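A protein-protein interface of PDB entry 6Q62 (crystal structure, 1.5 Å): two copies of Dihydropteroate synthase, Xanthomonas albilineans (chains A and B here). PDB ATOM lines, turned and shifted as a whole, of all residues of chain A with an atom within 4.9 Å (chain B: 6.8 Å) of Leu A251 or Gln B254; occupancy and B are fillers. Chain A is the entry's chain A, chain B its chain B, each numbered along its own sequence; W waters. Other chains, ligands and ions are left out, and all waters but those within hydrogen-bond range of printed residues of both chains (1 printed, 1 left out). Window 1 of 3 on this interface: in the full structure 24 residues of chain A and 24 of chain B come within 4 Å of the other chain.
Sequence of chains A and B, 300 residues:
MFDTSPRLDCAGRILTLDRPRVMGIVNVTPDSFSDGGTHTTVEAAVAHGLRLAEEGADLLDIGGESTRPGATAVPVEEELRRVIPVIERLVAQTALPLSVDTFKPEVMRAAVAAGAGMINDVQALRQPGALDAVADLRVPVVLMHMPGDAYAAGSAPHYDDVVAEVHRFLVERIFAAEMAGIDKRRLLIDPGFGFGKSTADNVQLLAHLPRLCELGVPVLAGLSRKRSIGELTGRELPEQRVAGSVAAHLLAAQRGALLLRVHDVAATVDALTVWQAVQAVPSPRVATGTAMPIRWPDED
Leu A206 touches Val B278. CA of Ala B271 touches CB of Ala A247, at 3.6 Å. Leu A251 touches Gln B254 (CD2 to NE2, 3.4 Å). CD1 of Leu A251 touches CG1 of Val B274, at 3.96 Å. Leu A251 touches Trp B275 (CD1 to CA, 3.7 Å). Leu A251 touches Val B278. Gln A254 touches Leu B251 (NE2 to CD2, 3.4 Å). Val B278 touches Arg A255.
Of the 10 printed residues of chain A, 5 touch a printed residue of chain B. Hydrophobic or aromatic side chains of chain A that line the printed part of chain B: Leu A206, Ala A247 and Leu A251. Hydrophobic or aromatic side chains of chain B within 4 Å of the printed part of chain A: Leu B251, Ala B271, Val B274, Trp B275 and Val B278. Among the printed residues, 9 pairs touch across the chains. Among the printed residues, no Asp or Glu carboxylate lies within 4 Å of a Lys or Arg side-chain nitrogen of the other chain.
Water W1 lies within hydrogen-bond range of NE2 of Gln A254 and NH2 of Arg B255.
Leu A251 touches just these residues of chain B: Gln B254, Val B274, Trp B275 and Val B278. His B249 touches none of the printed residues of chain A. Printed residues of chain A within 4 Å of Leu B251: Gln A254 (3.4 Å). Leu B272 touches none of the printed residues of chain A. Of the printed residues of chain A, Val B278 touches Leu A206 (3.7 Å), Leu A251 (3.9 Å) and Arg A255 (3.8 Å). The nearest residue of chain A that does not touch Gln B254 is Arg A255 (4.8 Å). The nearest printed residue of chain A that does not touch Trp B275 is Arg A255 (4.9 Å).
The side-chain amide nitrogen of Gln A254 sits at hydrogen-bond distance from the side-chain amide oxygen of Gln B254 (2.9 Å).
O of Leu A251 lies within hydrogen-bond range of NH1 of Arg A255.
Leu A251 touches Gln B254, and with the chains exchanged Gln A254 touches Leu B251. Gln A254 touches its own counterpart, Gln B254. Of the 9 pairs that touch across the chains among the printed residues, 3 have their exchanged pair printed and touching as well.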
ATOM      1  N   LEU A 206      27.707  10.289  11.697  1.00  0.00           N
ATOM      2  CA  LEU A 206      26.640  10.997  10.985  1.00  0.00           C
ATOM      3  C   LEU A 206      26.385  12.352  11.639  1.00  0.00           C
ATOM      4  O   LEU A 206      26.319  13.361  10.946  1.00  0.00           O
ATOM      5  CB  LEU A 206      25.346  10.164  10.968  1.00  0.00           C
ATOM      6  CG  LEU A 206      24.113  10.749  10.254  1.00  0.00           C
ATOM      7  CD1 LEU A 206      24.451  11.213   8.848  1.00  0.00           C
ATOM      8  CD2 LEU A 206      23.001   9.684  10.180  1.00  0.00           C
ATOM      9  N   ALA A 247      15.496   8.496   5.973  1.00  0.00           N
ATOM     10  CA  ALA A 247      15.712   9.523   6.984  1.00  0.00           C
ATOM     11  C   ALA A 247      17.222   9.736   7.182  1.00  0.00           C
ATOM     12  O   ALA A 247      17.673  10.880   7.171  1.00  0.00           O
ATOM     13  CB  ALA A 247      15.072   9.111   8.294  1.00  0.00           C
ATOM     14  N   ALA A 248      17.992   8.645   7.347  1.00  0.00           N
ATOM     15  CA  ALA A 248      19.460   8.731   7.529  1.00  0.00           C
ATOM     16  C   ALA A 248      20.145   9.457   6.356  1.00  0.00           C
ATOM     17  O   ALA A 248      20.983  10.340   6.575  1.00  0.00           O
ATOM     18  CB  ALA A 248      20.045   7.332   7.713  1.00  0.00           C
ATOM     19  N   HIS A 249      19.726   9.150   5.129  1.00  0.00           N
ATOM     20  CA  HIS A 249      20.297   9.805   3.953  1.00  0.00           C
ATOM     21  C   HIS A 249      19.931  11.269   3.860  1.00  0.00           C
ATOM     22  O   HIS A 249      20.788  12.091   3.510  1.00  0.00           O
ATOM     23  CB  HIS A 249      19.978   9.023   2.687  1.00  0.00           C
ATOM     24  CG  HIS A 249      20.756   7.735   2.665  1.00  0.00           C
ATOM     25  ND1 HIS A 249      20.130   6.513   2.614  1.00  0.00           N
ATOM     26  CD2 HIS A 249      22.097   7.537   2.771  1.00  0.00           C
ATOM     27  CE1 HIS A 249      21.099   5.605   2.654  1.00  0.00           C
ATOM     28  NE2 HIS A 249      22.301   6.181   2.773  1.00  0.00           N
ATOM     29  N   LEU A 250      18.684  11.626   4.225  1.00  0.00           N
ATOM     30  CA  LEU A 250      18.322  13.052   4.284  1.00  0.00           C
ATOM     31  C   LEU A 250      19.148  13.773   5.326  1.00  0.00           C
ATOM     32  O   LEU A 250      19.658  14.857   5.050  1.00  0.00           O
ATOM     33  CB  LEU A 250      16.813  13.176   4.588  1.00  0.00           C
ATOM     34  CG  LEU A 250      16.277  14.604   4.718  1.00  0.00           C
ATOM     35  CD1 LEU A 250      16.615  15.438   3.463  1.00  0.00           C
ATOM     36  CD2 LEU A 250      14.784  14.578   4.940  1.00  0.00           C
ATOM     37  N   LEU A 251      19.343  13.165   6.520  1.00  0.00           N
ATOM     38  CA  LEU A 251      20.172  13.773   7.559  1.00  0.00           C
ATOM     39  C   LEU A 251      21.612  13.946   7.081  1.00  0.00           C
ATOM     40  O   LEU A 251      22.214  14.991   7.332  1.00  0.00           O
ATOM     41  CB  LEU A 251      20.142  12.928   8.869  1.00  0.00           C
ATOM     42  CG  LEU A 251      18.789  12.851   9.568  1.00  0.00           C
ATOM     43  CD1 LEU A 251      18.859  11.859  10.726  1.00  0.00           C
ATOM     44  CD2 LEU A 251      18.329  14.252  10.053  1.00  0.00           C
ATOM     45  N   ALA A 252      22.144  12.959   6.328  1.00  0.00           N
ATOM     46  CA  ALA A 252      23.511  13.056   5.806  1.00  0.00           C
ATOM     47  C   ALA A 252      23.628  14.216   4.820  1.00  0.00           C
ATOM     48  O   ALA A 252      24.592  15.007   4.882  1.00  0.00           O
ATOM     49  CB  ALA A 252      23.898  11.739   5.119  1.00  0.00           C
ATOM     50  N   ALA A 253      22.647  14.337   3.924  1.00  0.00           N
ATOM     51  CA  ALA A 253      22.601  15.422   2.939  1.00  0.00           C
ATOM     52  C   ALA A 253      22.522  16.791   3.653  1.00  0.00           C
ATOM     53  O   ALA A 253      23.256  17.724   3.292  1.00  0.00           O
ATOM     54  CB  ALA A 253      21.405  15.228   2.031  1.00  0.00           C
ATOM     55  N   GLN A 254      21.708  16.895   4.713  1.00  0.00           N
ATOM     56  CA  GLN A 254      21.625  18.144   5.484  1.00  0.00           C
ATOM     57  C   GLN A 254      22.948  18.469   6.162  1.00  0.00           C
ATOM     58  O   GLN A 254      23.272  19.643   6.357  1.00  0.00           O
ATOM     59  CB  GLN A 254      20.534  18.013   6.553  1.00  0.00           C
ATOM     60  CG  GLN A 254      19.138  17.952   5.943  1.00  0.00           C
ATOM     61  CD  GLN A 254      18.096  17.778   7.003  1.00  0.00           C
ATOM     62  OE1 GLN A 254      18.320  17.125   8.038  1.00  0.00           O
ATOM     63  NE2 GLN A 254      16.932  18.380   6.775  1.00  0.00           N
ATOM     64  N   ARG A 255      23.738  17.418   6.496  1.00  0.00           N
ATOM     65  CA  ARG A 255      25.011  17.561   7.177  1.00  0.00           C
ATOM     66  C   ARG A 255      26.220  17.625   6.227  1.00  0.00           C
ATOM     67  O   ARG A 255      27.347  17.564   6.700  1.00  0.00           O
ATOM     68  CB  ARG A 255      25.174  16.494   8.261  1.00  0.00           C
ATOM     69  CG  ARG A 255      24.372  16.872   9.505  1.00  0.00           C
ATOM     70  CD  ARG A 255      23.925  15.708  10.355  1.00  0.00           C
ATOM     71  NE  ARG A 255      23.087  16.156  11.471  1.00  0.00           N
ATOM     72  CZ  ARG A 255      21.796  16.479  11.407  1.00  0.00           C
ATOM     73  NH1 ARG A 255      21.148  16.458  10.242  1.00  0.00           N
ATOM     74  NH2 ARG A 255      21.152  16.866  12.499  1.00  0.00           N
ATOM     75  N   PRO B  20       8.665  15.367  19.130  1.00  0.00           N
ATOM     76  CA  PRO B  20       7.536  15.295  18.181  1.00  0.00           C
ATOM     77  C   PRO B  20       6.781  13.963  18.301  1.00  0.00           C
ATOM     78  O   PRO B  20       7.390  12.894  18.387  1.00  0.00           O
ATOM     79  CB  PRO B  20       8.201  15.452  16.811  1.00  0.00           C
ATOM     80  CG  PRO B  20       9.511  16.123  17.090  1.00  0.00           C
ATOM     81  CD  PRO B  20       9.949  15.579  18.420  1.00  0.00           C
ATOM     82  N   PRO B 210       9.309  27.728  11.996  1.00  0.00           N
ATOM     83  CA  PRO B 210       9.759  28.214  13.304  1.00  0.00           C
ATOM     84  C   PRO B 210       9.072  29.511  13.756  1.00  0.00           C
ATOM     85  O   PRO B 210       8.890  29.698  14.950  1.00  0.00           O
ATOM     86  CB  PRO B 210      11.272  28.406  13.097  1.00  0.00           C
ATOM     87  CG  PRO B 210      11.629  27.433  12.038  1.00  0.00           C
ATOM     88  CD  PRO B 210      10.457  27.523  11.092  1.00  0.00           C
ATOM     89  N   ALA B 247       9.361  12.522   4.570  1.00  0.00           N
ATOM     90  CA  ALA B 247      10.399  13.565   4.522  1.00  0.00           C
ATOM     91  C   ALA B 247       9.822  14.902   5.014  1.00  0.00           C
ATOM     92  O   ALA B 247      10.455  15.553   5.827  1.00  0.00           O
ATOM     93  CB  ALA B 247      10.918  13.718   3.097  1.00  0.00           C
ATOM     94  N   HIS B 249       7.289  15.504   7.007  1.00  0.00           N
ATOM     95  CA  HIS B 249       7.051  15.437   8.456  1.00  0.00           C
ATOM     96  C   HIS B 249       8.316  15.493   9.276  1.00  0.00           C
ATOM     97  O   HIS B 249       8.337  16.205  10.289  1.00  0.00           O
ATOM     98  CB  HIS B 249       6.176  14.236   8.809  1.00  0.00           C
ATOM     99  CG  HIS B 249       4.758  14.468   8.342  1.00  0.00           C
ATOM    100  ND1 HIS B 249       4.143  13.603   7.477  1.00  0.00           N
ATOM    101  CD2 HIS B 249       3.910  15.498   8.607  1.00  0.00           C
ATOM    102  CE1 HIS B 249       2.941  14.112   7.241  1.00  0.00           C
ATOM    103  NE2 HIS B 249       2.757  15.255   7.894  1.00  0.00           N
ATOM    104  N   LEU B 250       9.410  14.892   8.785  1.00  0.00           N
ATOM    105  CA  LEU B 250      10.706  15.027   9.451  1.00  0.00           C
ATOM    106  C   LEU B 250      11.158  16.478   9.397  1.00  0.00           C
ATOM    107  O   LEU B 250      11.597  17.012  10.413  1.00  0.00           O
ATOM    108  CB  LEU B 250      11.758  14.097   8.805  1.00  0.00           C
ATOM    109  CG  LEU B 250      13.166  14.218   9.360  1.00  0.00           C
ATOM    110  CD1 LEU B 250      13.181  13.997  10.892  1.00  0.00           C
ATOM    111  CD2 LEU B 250      14.090  13.199   8.680  1.00  0.00           C
ATOM    112  N   LEU B 251      11.022  17.138   8.217  1.00  0.00           N
ATOM    113  CA  LEU B 251      11.404  18.546   8.080  1.00  0.00           C
ATOM    114  C   LEU B 251      10.573  19.427   9.014  1.00  0.00           C
ATOM    115  O   LEU B 251      11.129  20.319   9.648  1.00  0.00           O
ATOM    116  CB  LEU B 251      11.246  19.037   6.611  1.00  0.00           C
ATOM    117  CG  LEU B 251      12.189  18.354   5.595  1.00  0.00           C
ATOM    118  CD1 LEU B 251      11.856  18.765   4.206  1.00  0.00           C
ATOM    119  CD2 LEU B 251      13.662  18.650   5.890  1.00  0.00           C
ATOM    120  N   ALA B 252       9.271  19.147   9.145  1.00  0.00           N
ATOM    121  CA  ALA B 252       8.396  19.890  10.042  1.00  0.00           C
ATOM    122  C   ALA B 252       8.846  19.739  11.497  1.00  0.00           C
ATOM    123  O   ALA B 252       8.908  20.750  12.216  1.00  0.00           O
ATOM    124  CB  ALA B 252       6.956  19.425   9.889  1.00  0.00           C
ATOM    125  N   ALA B 253       9.187  18.507  11.908  1.00  0.00           N
ATOM    126  CA  ALA B 253       9.684  18.217  13.269  1.00  0.00           C
ATOM    127  C   ALA B 253      10.985  18.976  13.517  1.00  0.00           C
ATOM    128  O   ALA B 253      11.140  19.609  14.558  1.00  0.00           O
ATOM    129  CB  ALA B 253       9.894  16.733  13.439  1.00  0.00           C
ATOM    130  N   GLN B 254      11.906  18.975  12.529  1.00  0.00           N
ATOM    131  CA  GLN B 254      13.154  19.736  12.679  1.00  0.00           C
ATOM    132  C   GLN B 254      12.885  21.228  12.829  1.00  0.00           C
ATOM    133  O   GLN B 254      13.680  21.933  13.471  1.00  0.00           O
ATOM    134  CB  GLN B 254      14.046  19.519  11.440  1.00  0.00           C
ATOM    135  CG  GLN B 254      14.549  18.073  11.371  1.00  0.00           C
ATOM    136  CD  GLN B 254      15.373  17.841  10.145  1.00  0.00           C
ATOM    137  OE1 GLN B 254      15.097  18.374   9.073  1.00  0.00           O
ATOM    138  NE2 GLN B 254      16.428  17.050  10.297  1.00  0.00           N
ATOM    139  N   ARG B 255      11.799  21.720  12.195  1.00  0.00           N
ATOM    140  CA  ARG B 255      11.454  23.134  12.198  1.00  0.00           C
ATOM    141  C   ARG B 255      10.469  23.516  13.328  1.00  0.00           C
ATOM    142  O   ARG B 255       9.977  24.643  13.344  1.00  0.00           O
ATOM    143  CB  ARG B 255      10.976  23.583  10.815  1.00  0.00           C
ATOM    144  CG  ARG B 255      12.155  23.786   9.868  1.00  0.00           C
ATOM    145  CD  ARG B 255      11.800  23.683   8.404  1.00  0.00           C
ATOM    146  NE  ARG B 255      12.996  23.596   7.550  1.00  0.00           N
ATOM    147  CZ  ARG B 255      13.749  24.600   7.107  1.00  0.00           C
ATOM    148  NH1 ARG B 255      13.396  25.859   7.332  1.00  0.00           N
ATOM    149  NH2 ARG B 255      14.817  24.354   6.361  1.00  0.00           N
ATOM    150  N   GLY B 256      10.293  22.635  14.322  1.00  0.00           N
ATOM    151  CA  GLY B 256       9.539  22.996  15.520  1.00  0.00           C
ATOM    152  C   GLY B 256       8.205  22.325  15.745  1.00  0.00           C
ATOM    153  O   GLY B 256       7.662  22.434  16.849  1.00  0.00           O
ATOM    154  N   ALA B 257       7.670  21.613  14.739  1.00  0.00           N
ATOM    155  CA  ALA B 257       6.371  20.941  14.930  1.00  0.00           C
ATOM    156  C   ALA B 257       6.481  19.862  16.013  1.00  0.00           C
ATOM    157  O   ALA B 257       7.462  19.109  16.032  1.00  0.00           O
ATOM    158  CB  ALA B 257       5.875  20.326  13.630  1.00  0.00           C
ATOM    159  N   ALA B 271      11.539   7.319  10.882  1.00  0.00           N
ATOM    160  CA  ALA B 271      12.271   8.518  10.500  1.00  0.00           C
ATOM    161  C   ALA B 271      12.576   9.394  11.711  1.00  0.00           C
ATOM    162  O   ALA B 271      13.684   9.895  11.849  1.00  0.00           O
ATOM    163  CB  ALA B 271      11.477   9.315   9.471  1.00  0.00           C
ATOM    164  N   LEU B 272      11.587   9.591  12.601  1.00  0.00           N
ATOM    165  CA  LEU B 272      11.806  10.436  13.770  1.00  0.00           C
ATOM    166  C   LEU B 272      12.785   9.772  14.723  1.00  0.00           C
ATOM    167  O   LEU B 272      13.512  10.479  15.401  1.00  0.00           O
ATOM    168  CB  LEU B 272      10.477  10.676  14.497  1.00  0.00           C
ATOM    169  CG  LEU B 272       9.463  11.527  13.735  1.00  0.00           C
ATOM    170  CD1 LEU B 272       8.111  11.470  14.486  1.00  0.00           C
ATOM    171  CD2 LEU B 272       9.954  12.990  13.603  1.00  0.00           C
ATOM    172  N   VAL B 274      15.416   7.803  13.974  1.00  0.00           N
ATOM    173  CA  VAL B 274      16.775   7.992  13.439  1.00  0.00           C
ATOM    174  C   VAL B 274      17.216   9.425  13.741  1.00  0.00           C
ATOM    175  O   VAL B 274      18.317   9.627  14.256  1.00  0.00           O
ATOM    176  CB  VAL B 274      16.827   7.662  11.927  1.00  0.00           C
ATOM    177  CG1 VAL B 274      18.192   8.005  11.339  1.00  0.00           C
ATOM    178  CG2 VAL B 274      16.484   6.199  11.678  1.00  0.00           C
ATOM    179  N   TRP B 275      16.354  10.414  13.436  1.00  0.00           N
ATOM    180  CA  TRP B 275      16.646  11.814  13.722  1.00  0.00           C
ATOM    181  C   TRP B 275      16.912  12.059  15.205  1.00  0.00           C
ATOM    182  O   TRP B 275      17.902  12.739  15.519  1.00  0.00           O
ATOM    183  CB  TRP B 275      15.523  12.719  13.204  1.00  0.00           C
ATOM    184  CG  TRP B 275      15.650  14.152  13.625  1.00  0.00           C
ATOM    185  CD1 TRP B 275      16.675  15.013  13.352  1.00  0.00           C
ATOM    186  CD2 TRP B 275      14.711  14.877  14.410  1.00  0.00           C
ATOM    187  NE1 TRP B 275      16.432  16.233  13.935  1.00  0.00           N
ATOM    188  CE2 TRP B 275      15.219  16.186  14.570  1.00  0.00           C
ATOM    189  CE3 TRP B 275      13.481  14.547  14.999  1.00  0.00           C
ATOM    190  CZ2 TRP B 275      14.537  17.167  15.293  1.00  0.00           C
ATOM    191  CZ3 TRP B 275      12.800  15.524  15.714  1.00  0.00           C
ATOM    192  CH2 TRP B 275      13.327  16.817  15.848  1.00  0.00           C
ATOM    193  N   GLN B 276      16.071  11.491  16.109  1.00  0.00           N
ATOM    194  CA  GLN B 276      16.258  11.645  17.559  1.00  0.00           C
ATOM    195  C   GLN B 276      17.630  11.139  18.007  1.00  0.00           C
ATOM    196  O   GLN B 276      18.277  11.805  18.815  1.00  0.00           O
ATOM    197  CB  GLN B 276      15.148  10.944  18.355  1.00  0.00           C
ATOM    198  CG  GLN B 276      13.836  11.759  18.440  1.00  0.00           C
ATOM    199  CD  GLN B 276      13.932  12.996  19.292  1.00  0.00           C
ATOM    200  OE1 GLN B 276      14.223  12.941  20.495  1.00  0.00           O
ATOM    201  NE2 GLN B 276      13.670  14.137  18.688  1.00  0.00           N
ATOM    202  N   VAL B 278      20.439  10.962  16.214  1.00  0.00           N
ATOM    203  CA  VAL B 278      21.418  11.887  15.682  1.00  0.00           C
ATOM    204  C   VAL B 278      21.420  13.205  16.465  1.00  0.00           C
ATOM    205  O   VAL B 278      22.493  13.680  16.846  1.00  0.00           O
ATOM    206  CB  VAL B 278      21.196  12.097  14.160  1.00  0.00           C
ATOM    207  CG1 VAL B 278      22.051  13.225  13.618  1.00  0.00           C
ATOM    208  CG2 VAL B 278      21.464  10.806  13.392  1.00  0.00           C
ATOM    209  N   GLN B 279      20.228  13.788  16.697  1.00  0.00           N
ATOM    210  CA  GLN B 279      20.046  15.056  17.408  1.00  0.00           C
ATOM    211  C   GLN B 279      20.563  14.963  18.861  1.00  0.00           C
ATOM    212  O   GLN B 279      20.999  15.976  19.414  1.00  0.00           O
ATOM    213  CB  GLN B 279      18.554  15.453  17.383  1.00  0.00           C
ATOM    214  CG  GLN B 279      18.305  16.946  17.213  1.00  0.00           C
ATOM    215  CD  GLN B 279      17.072  17.440  17.946  1.00  0.00           C
ATOM    216  OE1 GLN B 279      16.439  16.729  18.739  1.00  0.00           O
ATOM    217  NE2 GLN B 279      16.712  18.688  17.706  1.00  0.00           N
HETATM  218  O   HOH W   1      16.786  21.693   6.742  1.00  0.00           O
